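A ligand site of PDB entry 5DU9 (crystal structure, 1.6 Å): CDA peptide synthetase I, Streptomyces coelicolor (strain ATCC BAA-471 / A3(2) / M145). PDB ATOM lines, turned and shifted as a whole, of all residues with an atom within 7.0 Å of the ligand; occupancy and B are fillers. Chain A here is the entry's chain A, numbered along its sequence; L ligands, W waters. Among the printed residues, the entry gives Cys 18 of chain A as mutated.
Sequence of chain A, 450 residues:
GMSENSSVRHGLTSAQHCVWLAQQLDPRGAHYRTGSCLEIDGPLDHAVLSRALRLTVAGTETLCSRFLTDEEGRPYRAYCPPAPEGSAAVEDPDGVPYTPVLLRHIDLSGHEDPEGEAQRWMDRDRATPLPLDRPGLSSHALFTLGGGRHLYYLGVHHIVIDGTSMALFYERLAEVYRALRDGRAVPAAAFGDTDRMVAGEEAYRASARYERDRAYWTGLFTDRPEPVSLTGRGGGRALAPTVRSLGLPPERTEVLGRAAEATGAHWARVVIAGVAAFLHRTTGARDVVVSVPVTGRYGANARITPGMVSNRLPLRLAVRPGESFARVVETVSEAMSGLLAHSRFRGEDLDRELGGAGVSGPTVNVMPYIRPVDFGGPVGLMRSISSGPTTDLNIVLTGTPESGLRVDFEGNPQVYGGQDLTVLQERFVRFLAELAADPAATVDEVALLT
CG2 of Val 19 touches C3 of the ligand (3.7 Å). Met 308 touches the ligand. Arg 312 touches the ligand (NH1 to C7, 3.7 Å). Glu 348 touches the ligand. Hydrophobic or aromatic side chains within 4 Å of the ligand: Val 19, His 158 and Met 308. Of the 27 residues printed, 7 come within 4 Å of the ligand. The nearest printed residue that does not touch the ligand is Ala 15 (4.03 Å).
The backbone carbonyl oxygen of Ser 387 lies within hydrogen-bond range of a nitrogen (N2) of the ligand, at 3.0 Å. NE2 of His 158 sits at hydrogen-bond distance from N2 of the ligand (2.8 Å). A carbon (C1) of the ligand is covalently linked to the side-chain sulfur (SG) of Cys 18 (1.8 Å).
Water W3 lies within hydrogen-bond range of O1 of the ligand (2.6 Å), O of Pro 389 (2.9 Å) and NH2 of Arg 312 (3.0 Å). Water W6 bridges a nitrogen (N1) of the ligand (2.8 Å) and the side-chain hydroxyl (OG) of Ser 310 (3.0 Å). Water W1 lies within hydrogen-bond range of N2 of the ligand (2.9 Å) and OG of Ser 387 (2.9 Å).
NH1 of Arg 312 lies within hydrogen-bond range of OG1 of Thr 363, at 2.9 Å. The backbone NH (N) of His 158 sits at hydrogen-bond distance from the backbone carbonyl oxygen (O) of Tyr 32, at 2.8 Å. The side-chain hydroxyl (OG) of Ser 310 sits at hydrogen-bond distance from the side-chain sulfur (SD) of Met 308. A ring nitrogen (ND1) of His 158 lies close to the side-chain sulfur (SD) of Met 308 (3.7 Å). The side-chain carboxylate of Glu 348 lies within salt-bridge range of the guanidinium group of Arg 346.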
ATOM      1  N   SER A  14      22.054  16.156  13.662  1.00  0.00           N
ATOM      2  CA  SER A  14      21.155  16.489  14.757  1.00  0.00           C
ATOM      3  C   SER A  14      21.844  17.380  15.778  1.00  0.00           C
ATOM      4  O   SER A  14      21.274  18.360  16.258  1.00  0.00           O
ATOM      5  CB  SER A  14      20.649  15.208  15.441  1.00  0.00           C
ATOM      6  OG  SER A  14      19.755  14.516  14.594  1.00  0.00           O
ATOM      7  N   ALA A  15      23.077  17.037  16.118  1.00  0.00           N
ATOM      8  CA  ALA A  15      23.849  17.815  17.088  1.00  0.00           C
ATOM      9  C   ALA A  15      24.087  19.230  16.583  1.00  0.00           C
ATOM     10  O   ALA A  15      24.032  20.186  17.339  1.00  0.00           O
ATOM     11  CB  ALA A  15      25.169  17.132  17.385  1.00  0.00           C
ATOM     12  N   GLN A  16      24.330  19.370  15.288  1.00  0.00           N
ATOM     13  CA  GLN A  16      24.545  20.690  14.713  1.00  0.00           C
ATOM     14  C   GLN A  16      23.254  21.505  14.735  1.00  0.00           C
ATOM     15  O   GLN A  16      23.286  22.710  15.021  1.00  0.00           O
ATOM     16  CB  GLN A  16      25.084  20.575  13.297  1.00  0.00           C
ATOM     17  CG  GLN A  16      26.532  20.137  13.257  1.00  0.00           C
ATOM     18  CD  GLN A  16      27.078  19.975  11.857  1.00  0.00           C
ATOM     19  OE1 GLN A  16      26.431  19.375  10.994  1.00  0.00           O
ATOM     20  NE2 GLN A  16      28.266  20.492  11.613  1.00  0.00           N
ATOM     21  N   HIS A  17      22.129  20.864  14.434  1.00  0.00           N
ATOM     22  CA  HIS A  17      20.821  21.519  14.545  1.00  0.00           C
ATOM     23  C   HIS A  17      20.593  22.030  15.972  1.00  0.00           C
ATOM     24  O   HIS A  17      20.066  23.119  16.178  1.00  0.00           O
ATOM     25  CB  HIS A  17      19.692  20.568  14.161  1.00  0.00           C
ATOM     26  CG  HIS A  17      19.411  20.509  12.687  1.00  0.00           C
ATOM     27  ND1 HIS A  17      18.844  21.564  11.996  1.00  0.00           N
ATOM     28  CD2 HIS A  17      19.596  19.527  11.770  1.00  0.00           C
ATOM     29  CE1 HIS A  17      18.705  21.240  10.726  1.00  0.00           C
ATOM     30  NE2 HIS A  17      19.155  20.006  10.564  1.00  0.00           N
ATOM     31  N   CYS A  18      20.997  21.223  16.945  1.00  0.00           N
ATOM     32  CA  CYS A  18      20.837  21.568  18.356  1.00  0.00           C
ATOM     33  C   CYS A  18      21.637  22.826  18.713  1.00  0.00           C
ATOM     34  O   CYS A  18      21.129  23.756  19.354  1.00  0.00           O
ATOM     35  CB  CYS A  18      21.282  20.393  19.236  1.00  0.00           C
ATOM     36  SG  CYS A  18      21.235  20.709  21.021  1.00  0.00           S
ATOM     37  N   VAL A  19      22.900  22.852  18.302  1.00  0.00           N
ATOM     38  CA  VAL A  19      23.757  24.005  18.554  1.00  0.00           C
ATOM     39  C   VAL A  19      23.225  25.233  17.823  1.00  0.00           C
ATOM     40  O   VAL A  19      23.208  26.322  18.383  1.00  0.00           O
ATOM     41  CB  VAL A  19      25.210  23.720  18.142  1.00  0.00           C
ATOM     42  CG1 VAL A  19      26.074  24.981  18.240  1.00  0.00           C
ATOM     43  CG2 VAL A  19      25.796  22.616  19.012  1.00  0.00           C
ATOM     44  N   ALA A  22      20.306  26.654  19.690  1.00  0.00           N
ATOM     45  CA  ALA A  22      20.738  27.209  20.960  1.00  0.00           C
ATOM     46  C   ALA A  22      21.457  28.537  20.747  1.00  0.00           C
ATOM     47  O   ALA A  22      21.329  29.471  21.552  1.00  0.00           O
ATOM     48  CB  ALA A  22      21.642  26.233  21.681  1.00  0.00           C
ATOM     49  N   TYR A  32      28.891  28.825  23.031  1.00  0.00           N
ATOM     50  CA  TYR A  32      29.186  27.557  22.379  1.00  0.00           C
ATOM     51  C   TYR A  32      30.589  27.544  21.760  1.00  0.00           C
ATOM     52  O   TYR A  32      30.895  26.700  20.914  1.00  0.00           O
ATOM     53  CB  TYR A  32      28.097  27.237  21.343  1.00  0.00           C
ATOM     54  CG  TYR A  32      26.849  26.709  22.019  1.00  0.00           C
ATOM     55  CD1 TYR A  32      25.883  27.574  22.519  1.00  0.00           C
ATOM     56  CD2 TYR A  32      26.664  25.348  22.208  1.00  0.00           C
ATOM     57  CE1 TYR A  32      24.762  27.102  23.176  1.00  0.00           C
ATOM     58  CE2 TYR A  32      25.545  24.860  22.847  1.00  0.00           C
ATOM     59  CZ  TYR A  32      24.594  25.737  23.326  1.00  0.00           C
ATOM     60  OH  TYR A  32      23.481  25.257  23.974  1.00  0.00           O
ATOM     61  N   THR A  34      34.150  26.312  22.311  1.00  0.00           N
ATOM     62  CA  THR A  34      34.798  25.252  23.068  1.00  0.00           C
ATOM     63  C   THR A  34      36.267  25.177  22.682  1.00  0.00           C
ATOM     64  O   THR A  34      36.692  25.848  21.746  1.00  0.00           O
ATOM     65  CB  THR A  34      34.122  23.894  22.812  1.00  0.00           C
ATOM     66  OG1 THR A  34      34.088  23.640  21.408  1.00  0.00           O
ATOM     67  CG2 THR A  34      32.695  23.909  23.339  1.00  0.00           C
ATOM     68  N   HIS A 158      31.394  24.994  18.734  1.00  0.00           N
ATOM     69  CA  HIS A 158      30.946  23.626  18.947  1.00  0.00           C
ATOM     70  C   HIS A 158      30.191  23.068  17.739  1.00  0.00           C
ATOM     71  O   HIS A 158      30.132  21.852  17.544  1.00  0.00           O
ATOM     72  CB  HIS A 158      30.080  23.546  20.207  1.00  0.00           C
ATOM     73  CG  HIS A 158      30.114  22.212  20.880  1.00  0.00           C
ATOM     74  ND1 HIS A 158      30.492  21.059  20.228  1.00  0.00           N
ATOM     75  CD2 HIS A 158      29.855  21.849  22.161  1.00  0.00           C
ATOM     76  CE1 HIS A 158      30.440  20.046  21.078  1.00  0.00           C
ATOM     77  NE2 HIS A 158      30.051  20.502  22.250  1.00  0.00           N
ATOM     78  N   ASP A 162      33.412  18.430  17.644  1.00  0.00           N
ATOM     79  CA  ASP A 162      33.170  17.784  18.941  1.00  0.00           C
ATOM     80  C   ASP A 162      34.453  17.168  19.490  1.00  0.00           C
ATOM     81  O   ASP A 162      35.521  17.274  18.875  1.00  0.00           O
ATOM     82  CB  ASP A 162      32.062  16.732  18.833  1.00  0.00           C
ATOM     83  CG  ASP A 162      32.294  15.706  17.733  1.00  0.00           C
ATOM     84  OD1 ASP A 162      33.466  15.422  17.406  1.00  0.00           O
ATOM     85  OD2 ASP A 162      31.300  15.161  17.215  1.00  0.00           O
ATOM     86  N   GLY A 163      34.361  16.536  20.653  1.00  0.00           N
ATOM     87  CA  GLY A 163      35.537  15.989  21.307  1.00  0.00           C
ATOM     88  C   GLY A 163      36.284  14.980  20.469  1.00  0.00           C
ATOM     89  O   GLY A 163      37.514  15.031  20.376  1.00  0.00           O
ATOM     90  N   PRO A 293      27.820  11.722  27.860  1.00  0.00           N
ATOM     91  CA  PRO A 293      27.959  11.898  26.403  1.00  0.00           C
ATOM     92  C   PRO A 293      28.280  10.586  25.687  1.00  0.00           C
ATOM     93  O   PRO A 293      28.965   9.727  26.229  1.00  0.00           O
ATOM     94  CB  PRO A 293      29.131  12.886  26.281  1.00  0.00           C
ATOM     95  CG  PRO A 293      29.864  12.827  27.574  1.00  0.00           C
ATOM     96  CD  PRO A 293      29.053  12.076  28.588  1.00  0.00           C
ATOM     97  N   MET A 308      30.402  17.581  14.255  1.00  0.00           N
ATOM     98  CA  MET A 308      29.717  17.690  15.522  1.00  0.00           C
ATOM     99  C   MET A 308      28.489  16.786  15.469  1.00  0.00           C
ATOM    100  O   MET A 308      27.518  17.117  14.783  1.00  0.00           O
ATOM    101  CB  MET A 308      29.320  19.146  15.802  1.00  0.00           C
ATOM    102  CG  MET A 308      28.269  19.347  16.874  1.00  0.00           C
ATOM    103  SD  MET A 308      28.642  18.465  18.399  1.00  0.00           S
ATOM    104  CE  MET A 308      27.580  19.340  19.558  1.00  0.00           C
ATOM    105  N   SER A 310      27.904  14.561  18.527  1.00  0.00           N
ATOM    106  CA  SER A 310      27.773  13.992  19.862  1.00  0.00           C
ATOM    107  C   SER A 310      26.368  14.158  20.452  1.00  0.00           C
ATOM    108  O   SER A 310      25.634  15.092  20.120  1.00  0.00           O
ATOM    109  CB  SER A 310      28.805  14.612  20.796  1.00  0.00           C
ATOM    110  OG  SER A 310      28.678  16.013  20.837  1.00  0.00           O
ATOM    111  N   ASN A 311      26.036  13.223  21.326  1.00  0.00           N
ATOM    112  CA  ASN A 311      24.731  13.154  21.972  1.00  0.00           C
ATOM    113  C   ASN A 311      24.962  13.111  23.485  1.00  0.00           C
ATOM    114  O   ASN A 311      26.020  12.708  23.933  1.00  0.00           O
ATOM    115  CB  ASN A 311      23.968  11.923  21.483  1.00  0.00           C
ATOM    116  CG  ASN A 311      22.507  11.934  21.867  1.00  0.00           C
ATOM    117  OD1 ASN A 311      21.895  12.980  22.073  1.00  0.00           O
ATOM    118  ND2 ASN A 311      21.915  10.754  21.937  1.00  0.00           N
ATOM    119  N   ARG A 312      23.974  13.552  24.249  1.00  0.00           N
ATOM    120  CA  ARG A 312      24.039  13.485  25.704  1.00  0.00           C
ATOM    121  C   ARG A 312      22.758  12.883  26.237  1.00  0.00           C
ATOM    122  O   ARG A 312      21.677  13.373  25.918  1.00  0.00           O
ATOM    123  CB  ARG A 312      24.269  14.867  26.304  1.00  0.00           C
ATOM    124  CG  ARG A 312      24.208  14.899  27.820  1.00  0.00           C
ATOM    125  CD  ARG A 312      24.883  16.137  28.374  1.00  0.00           C
ATOM    126  NE  ARG A 312      24.404  17.347  27.720  1.00  0.00           N
ATOM    127  CZ  ARG A 312      24.962  18.547  27.857  1.00  0.00           C
ATOM    128  NH1 ARG A 312      26.040  18.705  28.630  1.00  0.00           N
ATOM    129  NH2 ARG A 312      24.463  19.594  27.212  1.00  0.00           N
ATOM    130  N   ARG A 346      17.954  11.391  20.426  1.00  0.00           N
ATOM    131  CA  ARG A 346      18.626  12.634  20.787  1.00  0.00           C
ATOM    132  C   ARG A 346      18.203  13.136  22.162  1.00  0.00           C
ATOM    133  O   ARG A 346      17.029  13.184  22.479  1.00  0.00           O
ATOM    134  CB  ARG A 346      18.334  13.719  19.746  1.00  0.00           C
ATOM    135  CG  ARG A 346      18.861  13.394  18.354  1.00  0.00           C
ATOM    136  CD  ARG A 346      20.380  13.265  18.331  1.00  0.00           C
ATOM    137  NE  ARG A 346      21.028  14.459  18.878  1.00  0.00           N
ATOM    138  CZ  ARG A 346      22.333  14.595  19.052  1.00  0.00           C
ATOM    139  NH1 ARG A 346      23.178  13.622  18.720  1.00  0.00           N
ATOM    140  NH2 ARG A 346      22.800  15.726  19.566  1.00  0.00           N
ATOM    141  N   GLY A 347      19.190  13.512  22.973  1.00  0.00           N
ATOM    142  CA  GLY A 347      18.911  14.011  24.307  1.00  0.00           C
ATOM    143  C   GLY A 347      18.027  15.237  24.273  1.00  0.00           C
ATOM    144  O   GLY A 347      17.132  15.396  25.107  1.00  0.00           O
ATOM    145  N   GLU A 348      18.259  16.108  23.300  1.00  0.00           N
ATOM    146  CA  GLU A 348      17.485  17.335  23.201  1.00  0.00           C
ATOM    147  C   GLU A 348      16.057  17.049  22.746  1.00  0.00           C
ATOM    148  O   GLU A 348      15.141  17.810  23.040  1.00  0.00           O
ATOM    149  CB  GLU A 348      18.174  18.335  22.251  1.00  0.00           C
ATOM    150  CG  GLU A 348      18.282  17.897  20.787  1.00  0.00           C
ATOM    151  CD  GLU A 348      19.505  17.059  20.481  1.00  0.00           C
ATOM    152  OE1 GLU A 348      20.210  16.614  21.418  1.00  0.00           O
ATOM    153  OE2 GLU A 348      19.764  16.841  19.283  1.00  0.00           O
ATOM    154  N   THR A 363      27.157  16.482  33.840  1.00  0.00           N
ATOM    155  CA  THR A 363      27.689  15.721  32.725  1.00  0.00           C
ATOM    156  C   THR A 363      28.993  15.077  33.157  1.00  0.00           C
ATOM    157  O   THR A 363      29.904  15.769  33.601  1.00  0.00           O
ATOM    158  CB  THR A 363      27.916  16.594  31.480  1.00  0.00           C
ATOM    159  OG1 THR A 363      26.676  17.163  31.061  1.00  0.00           O
ATOM    160  CG2 THR A 363      28.508  15.761  30.347  1.00  0.00           C
ATOM    161  N   ASN A 365      31.988  13.217  31.703  1.00  0.00           N
ATOM    162  CA  ASN A 365      32.655  13.001  30.428  1.00  0.00           C
ATOM    163  C   ASN A 365      34.048  12.437  30.644  1.00  0.00           C
ATOM    164  O   ASN A 365      35.009  13.189  30.820  1.00  0.00           O
ATOM    165  CB  ASN A 365      32.725  14.338  29.660  1.00  0.00           C
ATOM    166  CG  ASN A 365      33.367  14.210  28.302  1.00  0.00           C
ATOM    167  OD1 ASN A 365      33.641  13.114  27.829  1.00  0.00           O
ATOM    168  ND2 ASN A 365      33.596  15.344  27.660  1.00  0.00           N
ATOM    169  N   SER A 387      34.671  22.158  27.403  1.00  0.00           N
ATOM    170  CA  SER A 387      33.984  21.114  26.633  1.00  0.00           C
ATOM    171  C   SER A 387      32.618  21.547  26.112  1.00  0.00           C
ATOM    172  O   SER A 387      32.080  20.908  25.210  1.00  0.00           O
ATOM    173  CB  SER A 387      33.837  19.842  27.478  1.00  0.00           C
ATOM    174  OG  SER A 387      32.774  19.949  28.420  1.00  0.00           O
ATOM    175  N   GLY A 388      32.064  22.614  26.662  1.00  0.00           N
ATOM    176  CA  GLY A 388      30.762  23.102  26.230  1.00  0.00           C
ATOM    177  C   GLY A 388      30.047  23.846  27.335  1.00  0.00           C
ATOM    178  O   GLY A 388      30.447  23.767  28.500  1.00  0.00           O
ATOM    179  N   PRO A 389      28.977  24.573  26.978  1.00  0.00           N
ATOM    180  CA  PRO A 389      28.231  25.326  27.990  1.00  0.00           C
ATOM    181  C   PRO A 389      27.416  24.404  28.893  1.00  0.00           C
ATOM    182  O   PRO A 389      27.148  23.269  28.503  1.00  0.00           O
ATOM    183  CB  PRO A 389      27.308  26.217  27.156  1.00  0.00           C
ATOM    184  CG  PRO A 389      27.112  25.458  25.896  1.00  0.00           C
ATOM    185  CD  PRO A 389      28.394  24.735  25.640  1.00  0.00           C
ATOM    186  N   THR A 390      27.034  24.895  30.060  1.00  0.00           N
ATOM    187  CA  THR A 390      26.306  24.073  31.017  1.00  0.00           C
ATOM    188  C   THR A 390      25.335  24.907  31.843  1.00  0.00           C
ATOM    189  O   THR A 390      25.567  26.085  32.125  1.00  0.00           O
ATOM    190  CB  THR A 390      27.284  23.332  31.956  1.00  0.00           C
ATOM    191  OG1 THR A 390      26.553  22.481  32.855  1.00  0.00           O
ATOM    192  CG2 THR A 390      28.134  24.303  32.755  1.00  0.00           C
ATOM    193  N   ASN A 394      29.770  20.331  34.358  1.00  0.00           N
ATOM    194  CA  ASN A 394      30.393  19.240  33.613  1.00  0.00           C
ATOM    195  C   ASN A 394      31.596  18.758  34.392  1.00  0.00           C
ATOM    196  O   ASN A 394      32.350  19.568  34.933  1.00  0.00           O
ATOM    197  CB  ASN A 394      30.878  19.669  32.216  1.00  0.00           C
ATOM    198  CG  ASN A 394      29.821  20.384  31.417  1.00  0.00           C
ATOM    199  OD1 ASN A 394      28.659  20.008  31.413  1.00  0.00           O
ATOM    200  ND2 ASN A 394      30.248  21.432  30.697  1.00  0.00           N
HETATM  201  C1  LIG L   1      22.360  19.581  21.876  1.00  0.00           C
HETATM  202  C2  LIG L   1      23.773  19.662  21.326  1.00  0.00           C
HETATM  203  C3  LIG L   1      24.600  20.759  21.987  1.00  0.00           C
HETATM  204  C4  LIG L   1      25.187  20.343  23.336  1.00  0.00           C
HETATM  205  N1  LIG L   1      26.425  19.589  23.243  1.00  0.00           N
HETATM  206  C5  LIG L   1      27.456  19.810  24.066  1.00  0.00           C
HETATM  207  O1  LIG L   1      27.653  20.885  24.610  1.00  0.00           O
HETATM  208  C6  LIG L   1      28.375  18.649  24.337  1.00  0.00           C
HETATM  209  C7  LIG L   1      27.839  17.850  25.514  1.00  0.00           C
HETATM  210  N2  LIG L   1      29.721  19.134  24.681  1.00  0.00           N
HETATM  211  O   HOH W   1      30.041  19.800  27.465  1.00  0.00           O
HETATM  212  O   HOH W   2      22.281  18.444  25.162  1.00  0.00           O
HETATM  213  O   HOH W   3      25.903  22.013  26.201  1.00  0.00           O
HETATM  214  O   HOH W   4      27.631  15.169  24.209  1.00  0.00           O
HETATM  215  O   HOH W   5      21.853  21.137  24.852  1.00  0.00           O
HETATM  216  O   HOH W   6      26.366  16.884  22.536  1.00  0.00           O
